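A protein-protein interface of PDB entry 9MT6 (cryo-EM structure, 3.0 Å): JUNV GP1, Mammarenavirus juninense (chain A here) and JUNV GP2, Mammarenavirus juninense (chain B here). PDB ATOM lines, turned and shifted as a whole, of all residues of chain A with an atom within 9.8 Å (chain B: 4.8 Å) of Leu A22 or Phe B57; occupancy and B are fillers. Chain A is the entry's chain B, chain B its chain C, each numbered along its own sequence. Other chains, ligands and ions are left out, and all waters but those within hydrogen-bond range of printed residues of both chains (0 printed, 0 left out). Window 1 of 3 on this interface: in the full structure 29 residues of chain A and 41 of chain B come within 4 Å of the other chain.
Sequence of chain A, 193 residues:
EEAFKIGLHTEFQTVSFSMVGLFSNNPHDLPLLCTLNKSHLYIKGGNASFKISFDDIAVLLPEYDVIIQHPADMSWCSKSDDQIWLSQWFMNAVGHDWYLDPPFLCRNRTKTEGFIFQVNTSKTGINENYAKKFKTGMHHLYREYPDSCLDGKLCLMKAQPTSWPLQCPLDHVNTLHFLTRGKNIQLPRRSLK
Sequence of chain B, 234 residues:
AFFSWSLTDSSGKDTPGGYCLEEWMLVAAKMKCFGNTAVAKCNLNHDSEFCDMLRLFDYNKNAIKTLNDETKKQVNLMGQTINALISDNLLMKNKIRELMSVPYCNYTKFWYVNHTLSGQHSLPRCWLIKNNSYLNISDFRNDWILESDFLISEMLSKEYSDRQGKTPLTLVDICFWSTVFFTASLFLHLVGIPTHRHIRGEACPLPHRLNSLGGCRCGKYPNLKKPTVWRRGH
O of Met B25 lies within hydrogen-bond range of N of Ser A18, 3.2 Å away.
The side-chain amide nitrogen (ND2) of Asn B60 is in hydrogen-bond range of the backbone carbonyl oxygen (O) of Asn A25 (2.4 Å).
SD of Met B53 lies within hydrogen-bond range of NE2 of His A172, at 3.4 Å.
The side-chain sulfur (SD) of Met A19 sits close to a ring nitrogen (ND1) of His A172 (3.5 Å).
O of Gly A21 is in hydrogen-bond range of OG of Ser A24, 2.8 Å away.
The side-chain amide oxygen of Asn A25 sits close to the backbone carbonyl oxygen of Gly A21 (3.0 Å).
OG of Ser A24 sits at hydrogen-bond distance from OD1 of Asn A25 (3.4 Å).
ND2 of Asn A26 sits at hydrogen-bond distance from O of His A28 (2.4 Å).
The side-chain amide nitrogen of Asn A26 sits close to the backbone NH of Leu A30, 3.5 Å away.
Among the printed residues, pairs that only touch across the chains: Phe A17 with Met B25, Phe A17 with Met B53, Phe A17 with Phe B57, Ser A18 with Trp B24, Ser A18 with Phe B57, Gly A21 with Trp B24, Leu A22 with Phe B57, Leu A22 with Asn B60, Asn A25 with Trp B24, Asn A26 with Asn B60 and Pro A27 with Asn B60.
Of chain B, only Phe B57 and Asn B60 come within 4 Å of Leu A22.
Phe B57 touches just these residues of chain A: Phe A17, Ser A18 and Leu A22.
Met B25 touches just these residues of chain A: Phe A17 and Ser A18.
No residue of chain A comes within 4 Å of Leu B56.
Of the printed residues of chain B, Gly A21 touches Trp B24 (3.97 Å).
Of the printed residues of chain B, Asn A25 touches Trp B24 (3.1 Å) and Asn B60 (2.4 Å).
Of the printed residues of chain B, Pro A27 touches Asn B60.
Printed residues of chain B within 4 Å of Ser A18: Trp B24 (3.7 Å), Met B25 (3.2 Å) and Phe B57 (3.4 Å).
Of the printed residues of chain B, Phe A17 touches Met B25 (3.3 Å), Met B53 (3.5 Å) and Phe B57 (3.9 Å).
The nearest printed residue of chain B that does not touch Leu A22 is Leu B56 (4.8 Å).
The nearest residue of chain A that does not touch Phe B57 is Met A19 (5.1 Å).
The nearest printed residue of chain B that does not touch Asn A25 is Lys B61 (6.5 Å).
Printed residues of chain A that touch a printed residue of chain B: Phe A17, Ser A18, Gly A21, Leu A22, Asn A25, Asn A26, Pro A27 and His A172.
Along chain A the printed residues that touch a printed residue of chain B span positions 17 to 172.
Printed residues of chain B that touch a printed residue of chain A: Trp B24, Met B25, Met B53, Phe B57 and Asn B60.
Hydrophobic or aromatic side chains of chain B within 4 Å of the printed part of chain A: Trp B24, Met B53 and Phe B57.
Along chain B the printed residues that touch a printed residue of chain A span positions 24 to 60.
Among the printed residues, 14 pairs touch across the chains.
Among the printed residues, no Asp or Glu carboxylate lies within 4 Å of a Lys or Arg side-chain nitrogen of the other chain.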
ATOM      1  N   SER A  16      33.088 -12.110 -21.760  1.00  0.00           N
ATOM      2  CA  SER A  16      32.500 -11.464 -20.597  1.00  0.00           C
ATOM      3  C   SER A  16      31.110 -12.030 -20.350  1.00  0.00           C
ATOM      4  O   SER A  16      30.316 -12.177 -21.284  1.00  0.00           O
ATOM      5  CB  SER A  16      32.425  -9.946 -20.780  1.00  0.00           C
ATOM      6  OG  SER A  16      32.195  -9.292 -19.546  1.00  0.00           O
ATOM      7  N   PHE A  17      30.823 -12.346 -19.094  1.00  0.00           N
ATOM      8  CA  PHE A  17      29.559 -12.952 -18.703  1.00  0.00           C
ATOM      9  C   PHE A  17      28.546 -11.872 -18.358  1.00  0.00           C
ATOM     10  O   PHE A  17      28.890 -10.869 -17.724  1.00  0.00           O
ATOM     11  CB  PHE A  17      29.743 -13.884 -17.508  1.00  0.00           C
ATOM     12  CG  PHE A  17      30.339 -15.212 -17.856  1.00  0.00           C
ATOM     13  CD1 PHE A  17      29.558 -16.214 -18.397  1.00  0.00           C
ATOM     14  CD2 PHE A  17      31.674 -15.467 -17.619  1.00  0.00           C
ATOM     15  CE1 PHE A  17      30.103 -17.441 -18.707  1.00  0.00           C
ATOM     16  CE2 PHE A  17      32.222 -16.690 -17.928  1.00  0.00           C
ATOM     17  CZ  PHE A  17      31.437 -17.678 -18.472  1.00  0.00           C
ATOM     18  N   SER A  18      27.301 -12.081 -18.775  1.00  0.00           N
ATOM     19  CA  SER A  18      26.210 -11.177 -18.448  1.00  0.00           C
ATOM     20  C   SER A  18      25.534 -11.639 -17.166  1.00  0.00           C
ATOM     21  O   SER A  18      25.289 -12.836 -16.980  1.00  0.00           O
ATOM     22  CB  SER A  18      25.197 -11.110 -19.590  1.00  0.00           C
ATOM     23  OG  SER A  18      24.124 -10.244 -19.270  1.00  0.00           O
ATOM     24  N   MET A  19      25.237 -10.689 -16.282  1.00  0.00           N
ATOM     25  CA  MET A  19      24.626 -10.990 -14.996  1.00  0.00           C
ATOM     26  C   MET A  19      23.125 -10.765 -14.996  1.00  0.00           C
ATOM     27  O   MET A  19      22.403 -11.443 -14.254  1.00  0.00           O
ATOM     28  CB  MET A  19      25.263 -10.128 -13.904  1.00  0.00           C
ATOM     29  CG  MET A  19      26.744 -10.368 -13.764  1.00  0.00           C
ATOM     30  SD  MET A  19      27.143 -12.083 -13.420  1.00  0.00           S
ATOM     31  CE  MET A  19      28.913 -12.018 -13.632  1.00  0.00           C
ATOM     32  N   VAL A  20      22.650  -9.821 -15.810  1.00  0.00           N
ATOM     33  CA  VAL A  20      21.215  -9.632 -15.983  1.00  0.00           C
ATOM     34  C   VAL A  20      20.579 -10.916 -16.487  1.00  0.00           C
ATOM     35  O   VAL A  20      19.528 -11.347 -15.992  1.00  0.00           O
ATOM     36  CB  VAL A  20      20.948  -8.458 -16.941  1.00  0.00           C
ATOM     37  CG1 VAL A  20      19.459  -8.312 -17.207  1.00  0.00           C
ATOM     38  CG2 VAL A  20      21.530  -7.172 -16.377  1.00  0.00           C
ATOM     39  N   GLY A  21      21.201 -11.544 -17.483  1.00  0.00           N
ATOM     40  CA  GLY A  21      20.694 -12.812 -17.974  1.00  0.00           C
ATOM     41  C   GLY A  21      20.748 -13.902 -16.924  1.00  0.00           C
ATOM     42  O   GLY A  21      19.843 -14.732 -16.836  1.00  0.00           O
ATOM     43  N   LEU A  22      21.801 -13.909 -16.108  1.00  0.00           N
ATOM     44  CA  LEU A  22      21.930 -14.937 -15.081  1.00  0.00           C
ATOM     45  C   LEU A  22      20.830 -14.817 -14.035  1.00  0.00           C
ATOM     46  O   LEU A  22      20.277 -15.828 -13.585  1.00  0.00           O
ATOM     47  CB  LEU A  22      23.306 -14.852 -14.423  1.00  0.00           C
ATOM     48  CG  LEU A  22      23.512 -15.691 -13.161  1.00  0.00           C
ATOM     49  CD1 LEU A  22      23.431 -17.172 -13.483  1.00  0.00           C
ATOM     50  CD2 LEU A  22      24.846 -15.355 -12.514  1.00  0.00           C
ATOM     51  N   PHE A  23      20.536 -13.574 -13.642  1.00  0.00           N
ATOM     52  CA  PHE A  23      19.507 -13.334 -12.595  1.00  0.00           C
ATOM     53  C   PHE A  23      18.116 -13.492 -13.209  1.00  0.00           C
ATOM     54  O   PHE A  23      17.222 -14.035 -12.531  1.00  0.00           O
ATOM     55  CB  PHE A  23      19.726 -11.945 -11.991  1.00  0.00           C
ATOM     56  CG  PHE A  23      20.764 -11.890 -10.878  1.00  0.00           C
ATOM     57  CD1 PHE A  23      20.515 -12.470  -9.639  1.00  0.00           C
ATOM     58  CD2 PHE A  23      21.987 -11.258 -11.072  1.00  0.00           C
ATOM     59  CE1 PHE A  23      21.461 -12.417  -8.627  1.00  0.00           C
ATOM     60  CE2 PHE A  23      22.929 -11.206 -10.057  1.00  0.00           C
ATOM     61  CZ  PHE A  23      22.665 -11.786  -8.837  1.00  0.00           C
ATOM     62  N   SER A  24      17.936 -13.024 -14.449  1.00  0.00           N
ATOM     63  CA  SER A  24      16.627 -13.171 -15.138  1.00  0.00           C
ATOM     64  C   SER A  24      16.243 -14.655 -15.175  1.00  0.00           C
ATOM     65  O   SER A  24      15.253 -15.029 -14.511  1.00  0.00           O
ATOM     66  CB  SER A  24      16.655 -12.578 -16.523  1.00  0.00           C
ATOM     67  OG  SER A  24      17.443 -13.367 -17.403  1.00  0.00           O
ATOM     68  N   ASN A  25      17.067 -15.459 -15.829  1.00  0.00           N
ATOM     69  CA  ASN A  25      16.815 -16.911 -15.931  1.00  0.00           C
ATOM     70  C   ASN A  25      17.259 -17.558 -14.638  1.00  0.00           C
ATOM     71  O   ASN A  25      18.466 -17.642 -14.428  1.00  0.00           O
ATOM     72  CB  ASN A  25      17.617 -17.531 -17.058  1.00  0.00           C
ATOM     73  CG  ASN A  25      17.392 -16.798 -18.359  1.00  0.00           C
ATOM     74  OD1 ASN A  25      18.328 -16.225 -18.924  1.00  0.00           O
ATOM     75  ND2 ASN A  25      16.159 -16.790 -18.840  1.00  0.00           N
ATOM     76  N   ASN A  26      16.320 -17.970 -13.799  1.00  0.00           N
ATOM     77  CA  ASN A  26      16.729 -18.530 -12.485  1.00  0.00           C
ATOM     78  C   ASN A  26      15.629 -19.425 -11.927  1.00  0.00           C
ATOM     79  O   ASN A  26      14.454 -19.017 -11.925  1.00  0.00           O
ATOM     80  CB  ASN A  26      17.128 -17.445 -11.492  1.00  0.00           C
ATOM     81  CG  ASN A  26      17.810 -18.031 -10.280  1.00  0.00           C
ATOM     82  OD1 ASN A  26      18.482 -19.063 -10.385  1.00  0.00           O
ATOM     83  ND2 ASN A  26      17.656 -17.387  -9.135  1.00  0.00           N
ATOM     84  N   PRO A  27      15.980 -20.630 -11.451  1.00  0.00           N
ATOM     85  CA  PRO A  27      15.000 -21.535 -10.800  1.00  0.00           C
ATOM     86  C   PRO A  27      14.568 -20.963  -9.452  1.00  0.00           C
ATOM     87  O   PRO A  27      13.527 -21.410  -8.921  1.00  0.00           O
ATOM     88  CB  PRO A  27      15.753 -22.859 -10.694  1.00  0.00           C
ATOM     89  CG  PRO A  27      17.212 -22.459 -10.635  1.00  0.00           C
ATOM     90  CD  PRO A  27      17.330 -21.267 -11.523  1.00  0.00           C
ATOM     91  N   HIS A  28      15.335 -20.021  -8.900  1.00  0.00           N
ATOM     92  CA  HIS A  28      15.001 -19.486  -7.564  1.00  0.00           C
ATOM     93  C   HIS A  28      15.089 -17.961  -7.570  1.00  0.00           C
ATOM     94  O   HIS A  28      15.306 -17.382  -8.640  1.00  0.00           O
ATOM     95  CB  HIS A  28      15.903 -20.102  -6.497  1.00  0.00           C
ATOM     96  CG  HIS A  28      16.099 -21.572  -6.630  1.00  0.00           C
ATOM     97  ND1 HIS A  28      15.056 -22.470  -6.619  1.00  0.00           N
ATOM     98  CD2 HIS A  28      17.214 -22.297  -6.774  1.00  0.00           C
ATOM     99  CE1 HIS A  28      15.538 -23.697  -6.757  1.00  0.00           C
ATOM    100  NE2 HIS A  28      16.847 -23.615  -6.850  1.00  0.00           N
ATOM    101  N   ASP A  29      14.896 -17.342  -6.407  1.00  0.00           N
ATOM    102  CA  ASP A  29      14.962 -15.863  -6.274  1.00  0.00           C
ATOM    103  C   ASP A  29      16.227 -15.523  -5.502  1.00  0.00           C
ATOM    104  O   ASP A  29      16.123 -15.178  -4.311  1.00  0.00           O
ATOM    105  CB  ASP A  29      13.766 -15.276  -5.554  1.00  0.00           C
ATOM    106  CG  ASP A  29      12.427 -15.529  -6.229  1.00  0.00           C
ATOM    107  OD1 ASP A  29      12.412 -15.623  -7.474  1.00  0.00           O
ATOM    108  OD2 ASP A  29      11.414 -15.633  -5.507  1.00  0.00           O
ATOM    109  N   LEU A  30      17.371 -15.620  -6.169  1.00  0.00           N
ATOM    110  CA  LEU A  30      18.666 -15.358  -5.521  1.00  0.00           C
ATOM    111  C   LEU A  30      18.616 -14.005  -4.815  1.00  0.00           C
ATOM    112  O   LEU A  30      18.095 -13.051  -5.414  1.00  0.00           O
ATOM    113  CB  LEU A  30      19.659 -15.387  -6.676  1.00  0.00           C
ATOM    114  CG  LEU A  30      19.858 -16.737  -7.371  1.00  0.00           C
ATOM    115  CD1 LEU A  30      21.090 -16.667  -8.254  1.00  0.00           C
ATOM    116  CD2 LEU A  30      20.004 -17.853  -6.356  1.00  0.00           C
ATOM    117  N   PRO A  31      19.147 -13.866  -3.588  1.00  0.00           N
ATOM    118  CA  PRO A  31      19.217 -12.562  -2.886  1.00  0.00           C
ATOM    119  C   PRO A  31      20.096 -11.561  -3.623  1.00  0.00           C
ATOM    120  O   PRO A  31      21.048 -12.002  -4.296  1.00  0.00           O
ATOM    121  CB  PRO A  31      19.791 -12.955  -1.544  1.00  0.00           C
ATOM    122  CG  PRO A  31      19.438 -14.417  -1.388  1.00  0.00           C
ATOM    123  CD  PRO A  31      19.702 -14.957  -2.738  1.00  0.00           C
ATOM    124  N   LEU A  32      19.805 -10.268  -3.539  1.00  0.00           N
ATOM    125  CA  LEU A  32      20.599  -9.211  -4.148  1.00  0.00           C
ATOM    126  C   LEU A  32      21.213  -8.341  -3.062  1.00  0.00           C
ATOM    127  O   LEU A  32      20.530  -7.956  -2.108  1.00  0.00           O
ATOM    128  CB  LEU A  32      19.758  -8.348  -5.089  1.00  0.00           C
ATOM    129  CG  LEU A  32      19.489  -8.840  -6.511  1.00  0.00           C
ATOM    130  CD1 LEU A  32      18.484  -9.970  -6.527  1.00  0.00           C
ATOM    131  CD2 LEU A  32      19.011  -7.691  -7.378  1.00  0.00           C
ATOM    132  N   LEU A 170      24.472  -4.850 -10.439  1.00  0.00           N
ATOM    133  CA  LEU A 170      23.899  -6.187 -10.321  1.00  0.00           C
ATOM    134  C   LEU A 170      24.982  -7.199  -9.980  1.00  0.00           C
ATOM    135  O   LEU A 170      25.144  -8.231 -10.634  1.00  0.00           O
ATOM    136  CB  LEU A 170      23.168  -6.574 -11.601  1.00  0.00           C
ATOM    137  CG  LEU A 170      22.061  -7.613 -11.440  1.00  0.00           C
ATOM    138  CD1 LEU A 170      21.234  -7.322 -10.203  1.00  0.00           C
ATOM    139  CD2 LEU A 170      21.181  -7.647 -12.674  1.00  0.00           C
ATOM    140  N   ASP A 171      25.749  -6.890  -8.940  1.00  0.00           N
ATOM    141  CA  ASP A 171      26.817  -7.770  -8.488  1.00  0.00           C
ATOM    142  C   ASP A 171      26.265  -9.137  -8.108  1.00  0.00           C
ATOM    143  O   ASP A 171      25.170  -9.253  -7.550  1.00  0.00           O
ATOM    144  CB  ASP A 171      27.529  -7.137  -7.295  1.00  0.00           C
ATOM    145  CG  ASP A 171      28.877  -7.752  -7.024  1.00  0.00           C
ATOM    146  OD1 ASP A 171      29.110  -8.909  -7.429  1.00  0.00           O
ATOM    147  OD2 ASP A 171      29.712  -7.070  -6.399  1.00  0.00           O
ATOM    148  N   HIS A 172      27.033 -10.184  -8.419  1.00  0.00           N
ATOM    149  CA  HIS A 172      26.633 -11.550  -8.116  1.00  0.00           C
ATOM    150  C   HIS A 172      27.583 -12.274  -7.175  1.00  0.00           C
ATOM    151  O   HIS A 172      27.211 -13.323  -6.643  1.00  0.00           O
ATOM    152  CB  HIS A 172      26.496 -12.368  -9.406  1.00  0.00           C
ATOM    153  CG  HIS A 172      27.762 -13.041  -9.833  1.00  0.00           C
ATOM    154  ND1 HIS A 172      28.828 -12.352 -10.368  1.00  0.00           N
ATOM    155  CD2 HIS A 172      28.131 -14.343  -9.805  1.00  0.00           C
ATOM    156  CE1 HIS A 172      29.801 -13.200 -10.647  1.00  0.00           C
ATOM    157  NE2 HIS A 172      29.403 -14.415 -10.316  1.00  0.00           N
ATOM    158  N   VAL A 173      28.793 -11.752  -6.964  1.00  0.00           N
ATOM    159  CA  VAL A 173      29.685 -12.326  -5.960  1.00  0.00           C
ATOM    160  C   VAL A 173      29.087 -12.160  -4.571  1.00  0.00           C
ATOM    161  O   VAL A 173      29.230 -13.033  -3.702  1.00  0.00           O
ATOM    162  CB  VAL A 173      31.079 -11.681  -6.054  1.00  0.00           C
ATOM    163  CG1 VAL A 173      32.078 -12.461  -5.226  1.00  0.00           C
ATOM    164  CG2 VAL A 173      31.530 -11.599  -7.500  1.00  0.00           C
ATOM    165  N   THR A 175      25.909 -12.220  -3.873  1.00  0.00           N
ATOM    166  CA  THR A 175      24.926 -13.289  -3.752  1.00  0.00           C
ATOM    167  C   THR A 175      25.601 -14.622  -3.458  1.00  0.00           C
ATOM    168  O   THR A 175      25.080 -15.432  -2.684  1.00  0.00           O
ATOM    169  CB  THR A 175      24.092 -13.378  -5.028  1.00  0.00           C
ATOM    170  OG1 THR A 175      23.376 -12.151  -5.217  1.00  0.00           O
ATOM    171  CG2 THR A 175      23.101 -14.524  -4.943  1.00  0.00           C
ATOM    172  N   LEU A 176      26.763 -14.866  -4.067  1.00  0.00           N
ATOM    173  CA  LEU A 176      27.473 -16.119  -3.826  1.00  0.00           C
ATOM    174  C   LEU A 176      27.909 -16.235  -2.372  1.00  0.00           C
ATOM    175  O   LEU A 176      27.726 -17.284  -1.742  1.00  0.00           O
ATOM    176  CB  LEU A 176      28.675 -16.226  -4.762  1.00  0.00           C
ATOM    177  CG  LEU A 176      28.343 -16.411  -6.243  1.00  0.00           C
ATOM    178  CD1 LEU A 176      29.604 -16.429  -7.085  1.00  0.00           C
ATOM    179  CD2 LEU A 176      27.540 -17.681  -6.451  1.00  0.00           C
ATOM    180  N   LEU A 179      24.783 -16.813  -0.172  1.00  0.00           N
ATOM    181  CA  LEU A 179      24.303 -18.190  -0.232  1.00  0.00           C
ATOM    182  C   LEU A 179      25.244 -19.136   0.500  1.00  0.00           C
ATOM    183  O   LEU A 179      24.792 -20.080   1.157  1.00  0.00           O
ATOM    184  CB  LEU A 179      24.124 -18.626  -1.684  1.00  0.00           C
ATOM    185  CG  LEU A 179      22.970 -17.981  -2.448  1.00  0.00           C
ATOM    186  CD1 LEU A 179      22.878 -18.545  -3.855  1.00  0.00           C
ATOM    187  CD2 LEU A 179      21.663 -18.176  -1.706  1.00  0.00           C
ATOM    188  N   TRP B  24      22.463 -15.114 -24.123  1.00  0.00           N
ATOM    189  CA  TRP B  24      22.132 -14.495 -22.841  1.00  0.00           C
ATOM    190  C   TRP B  24      23.205 -14.713 -21.786  1.00  0.00           C
ATOM    191  O   TRP B  24      23.229 -13.982 -20.792  1.00  0.00           O
ATOM    192  CB  TRP B  24      20.791 -15.027 -22.334  1.00  0.00           C
ATOM    193  CG  TRP B  24      20.711 -16.522 -22.271  1.00  0.00           C
ATOM    194  CD1 TRP B  24      20.417 -17.364 -23.300  1.00  0.00           C
ATOM    195  CD2 TRP B  24      20.904 -17.350 -21.118  1.00  0.00           C
ATOM    196  NE1 TRP B  24      20.425 -18.666 -22.865  1.00  0.00           N
ATOM    197  CE2 TRP B  24      20.719 -18.684 -21.529  1.00  0.00           C
ATOM    198  CE3 TRP B  24      21.216 -17.096 -19.780  1.00  0.00           C
ATOM    199  CZ2 TRP B  24      20.838 -19.758 -20.653  1.00  0.00           C
ATOM    200  CZ3 TRP B  24      21.333 -18.165 -18.912  1.00  0.00           C
ATOM    201  CH2 TRP B  24      21.145 -19.479 -19.352  1.00  0.00           C
ATOM    202  N   MET B  25      24.085 -15.691 -21.983  1.00  0.00           N
ATOM    203  CA  MET B  25      25.174 -15.977 -21.063  1.00  0.00           C
ATOM    204  C   MET B  25      26.315 -14.977 -21.176  1.00  0.00           C
ATOM    205  O   MET B  25      27.156 -14.915 -20.274  1.00  0.00           O
ATOM    206  CB  MET B  25      25.694 -17.387 -21.333  1.00  0.00           C
ATOM    207  CG  MET B  25      24.794 -18.487 -20.816  1.00  0.00           C
ATOM    208  SD  MET B  25      25.710 -19.949 -20.317  1.00  0.00           S
ATOM    209  CE  MET B  25      24.399 -21.163 -20.234  1.00  0.00           C
ATOM    210  N   MET B  53      32.142 -20.464 -13.125  1.00  0.00           N
ATOM    211  CA  MET B  53      31.075 -19.732 -13.795  1.00  0.00           C
ATOM    212  C   MET B  53      30.399 -20.595 -14.853  1.00  0.00           C
ATOM    213  O   MET B  53      29.175 -20.524 -15.030  1.00  0.00           O
ATOM    214  CB  MET B  53      31.629 -18.446 -14.397  1.00  0.00           C
ATOM    215  CG  MET B  53      31.937 -17.386 -13.355  1.00  0.00           C
ATOM    216  SD  MET B  53      30.524 -16.390 -12.860  1.00  0.00           S
ATOM    217  CE  MET B  53      29.953 -15.812 -14.447  1.00  0.00           C
ATOM    218  N   LEU B  54      31.173 -21.425 -15.557  1.00  0.00           N
ATOM    219  CA  LEU B  54      30.580 -22.377 -16.492  1.00  0.00           C
ATOM    220  C   LEU B  54      29.662 -23.351 -15.773  1.00  0.00           C
ATOM    221  O   LEU B  54      28.575 -23.661 -16.265  1.00  0.00           O
ATOM    222  CB  LEU B  54      31.659 -23.157 -17.241  1.00  0.00           C
ATOM    223  CG  LEU B  54      32.543 -22.483 -18.283  1.00  0.00           C
ATOM    224  CD1 LEU B  54      33.579 -23.480 -18.776  1.00  0.00           C
ATOM    225  CD2 LEU B  54      31.705 -21.960 -19.430  1.00  0.00           C
ATOM    226  N   ARG B  55      30.091 -23.860 -14.618  1.00  0.00           N
ATOM    227  CA  ARG B  55      29.244 -24.774 -13.859  1.00  0.00           C
ATOM    228  C   ARG B  55      27.943 -24.099 -13.450  1.00  0.00           C
ATOM    229  O   ARG B  55      26.857 -24.666 -13.619  1.00  0.00           O
ATOM    230  CB  ARG B  55      29.995 -25.282 -12.632  1.00  0.00           C
ATOM    231  CG  ARG B  55      30.782 -26.545 -12.871  1.00  0.00           C
ATOM    232  CD  ARG B  55      31.334 -27.094 -11.576  1.00  0.00           C
ATOM    233  NE  ARG B  55      32.421 -26.277 -11.056  1.00  0.00           N
ATOM    234  CZ  ARG B  55      33.688 -26.402 -11.423  1.00  0.00           C
ATOM    235  NH1 ARG B  55      34.060 -27.296 -12.323  1.00  0.00           N
ATOM    236  NH2 ARG B  55      34.604 -25.612 -10.872  1.00  0.00           N
ATOM    237  N   LEU B  56      28.036 -22.868 -12.945  1.00  0.00           N
ATOM    238  CA  LEU B  56      26.847 -22.137 -12.522  1.00  0.00           C
ATOM    239  C   LEU B  56      25.893 -21.912 -13.690  1.00  0.00           C
ATOM    240  O   LEU B  56      24.681 -22.139 -13.577  1.00  0.00           O
ATOM    241  CB  LEU B  56      27.261 -20.805 -11.898  1.00  0.00           C
ATOM    242  CG  LEU B  56      26.451 -20.244 -10.734  1.00  0.00           C
ATOM    243  CD1 LEU B  56      26.379 -21.241  -9.592  1.00  0.00           C
ATOM    244  CD2 LEU B  56      27.060 -18.936 -10.266  1.00  0.00           C
ATOM    245  N   PHE B  57      26.428 -21.486 -14.835  1.00  0.00           N
ATOM    246  CA  PHE B  57      25.564 -21.143 -15.958  1.00  0.00           C
ATOM    247  C   PHE B  57      24.995 -22.387 -16.628  1.00  0.00           C
ATOM    248  O   PHE B  57      23.850 -22.375 -17.093  1.00  0.00           O
ATOM    249  CB  PHE B  57      26.331 -20.288 -16.959  1.00  0.00           C
ATOM    250  CG  PHE B  57      26.183 -18.817 -16.733  1.00  0.00           C
ATOM    251  CD1 PHE B  57      26.973 -18.165 -15.810  1.00  0.00           C
ATOM    252  CD2 PHE B  57      25.249 -18.089 -17.437  1.00  0.00           C
ATOM    253  CE1 PHE B  57      26.840 -16.812 -15.602  1.00  0.00           C
ATOM    254  CE2 PHE B  57      25.112 -16.734 -17.235  1.00  0.00           C
ATOM    255  CZ  PHE B  57      25.908 -16.096 -16.314  1.00  0.00           C
ATOM    256  N   ASP B  58      25.775 -23.467 -16.694  1.00  0.00           N
ATOM    257  CA  ASP B  58      25.252 -24.729 -17.199  1.00  0.00           C
ATOM    258  C   ASP B  58      24.137 -25.238 -16.303  1.00  0.00           C
ATOM    259  O   ASP B  58      23.115 -25.734 -16.789  1.00  0.00           O
ATOM    260  CB  ASP B  58      26.379 -25.760 -17.295  1.00  0.00           C
ATOM    261  CG  ASP B  58      25.950 -27.049 -17.978  1.00  0.00           C
ATOM    262  OD1 ASP B  58      24.794 -27.141 -18.443  1.00  0.00           O
ATOM    263  OD2 ASP B  58      26.779 -27.980 -18.051  1.00  0.00           O
ATOM    264  N   TYR B  59      24.309 -25.108 -14.988  1.00  0.00           N
ATOM    265  CA  TYR B  59      23.251 -25.475 -14.056  1.00  0.00           C
ATOM    266  C   TYR B  59      21.987 -24.660 -14.302  1.00  0.00           C
ATOM    267  O   TYR B  59      20.878 -25.206 -14.334  1.00  0.00           O
ATOM    268  CB  TYR B  59      23.754 -25.277 -12.631  1.00  0.00           C
ATOM    269  CG  TYR B  59      22.732 -25.587 -11.581  1.00  0.00           C
ATOM    270  CD1 TYR B  59      22.443 -26.895 -11.234  1.00  0.00           C
ATOM    271  CD2 TYR B  59      22.049 -24.566 -10.941  1.00  0.00           C
ATOM    272  CE1 TYR B  59      21.509 -27.177 -10.275  1.00  0.00           C
ATOM    273  CE2 TYR B  59      21.115 -24.836  -9.982  1.00  0.00           C
ATOM    274  CZ  TYR B  59      20.849 -26.144  -9.654  1.00  0.00           C
ATOM    275  OH  TYR B  59      19.919 -26.428  -8.697  1.00  0.00           O
ATOM    276  N   ASN B  60      22.136 -23.346 -14.473  1.00  0.00           N
ATOM    277  CA  ASN B  60      20.971 -22.496 -14.706  1.00  0.00           C
ATOM    278  C   ASN B  60      20.270 -22.853 -16.014  1.00  0.00           C
ATOM    279  O   ASN B  60      19.037 -22.953 -16.060  1.00  0.00           O
ATOM    280  CB  ASN B  60      21.389 -21.027 -14.703  1.00  0.00           C
ATOM    281  CG  ASN B  60      20.206 -20.088 -14.688  1.00  0.00           C
ATOM    282  OD1 ASN B  60      19.143 -20.420 -14.164  1.00  0.00           O
ATOM    283  ND2 ASN B  60      20.381 -18.903 -15.262  1.00  0.00           N
ATOM    284  N   LYS B  61      21.039 -23.047 -17.089  1.00  0.00           N
ATOM    285  CA  LYS B  61      20.443 -23.373 -18.380  1.00  0.00           C
ATOM    286  C   LYS B  61      19.788 -24.748 -18.350  1.00  0.00           C
ATOM    287  O   LYS B  61      18.780 -24.980 -19.028  1.00  0.00           O
ATOM    288  CB  LYS B  61      21.504 -23.293 -19.480  1.00  0.00           C
ATOM    289  CG  LYS B  61      21.001 -23.582 -20.891  1.00  0.00           C
ATOM    290  CD  LYS B  61      21.241 -25.028 -21.303  1.00  0.00           C
ATOM    291  CE  LYS B  61      22.721 -25.307 -21.514  1.00  0.00           C
ATOM    292  NZ  LYS B  61      22.967 -26.720 -21.915  1.00  0.00           N
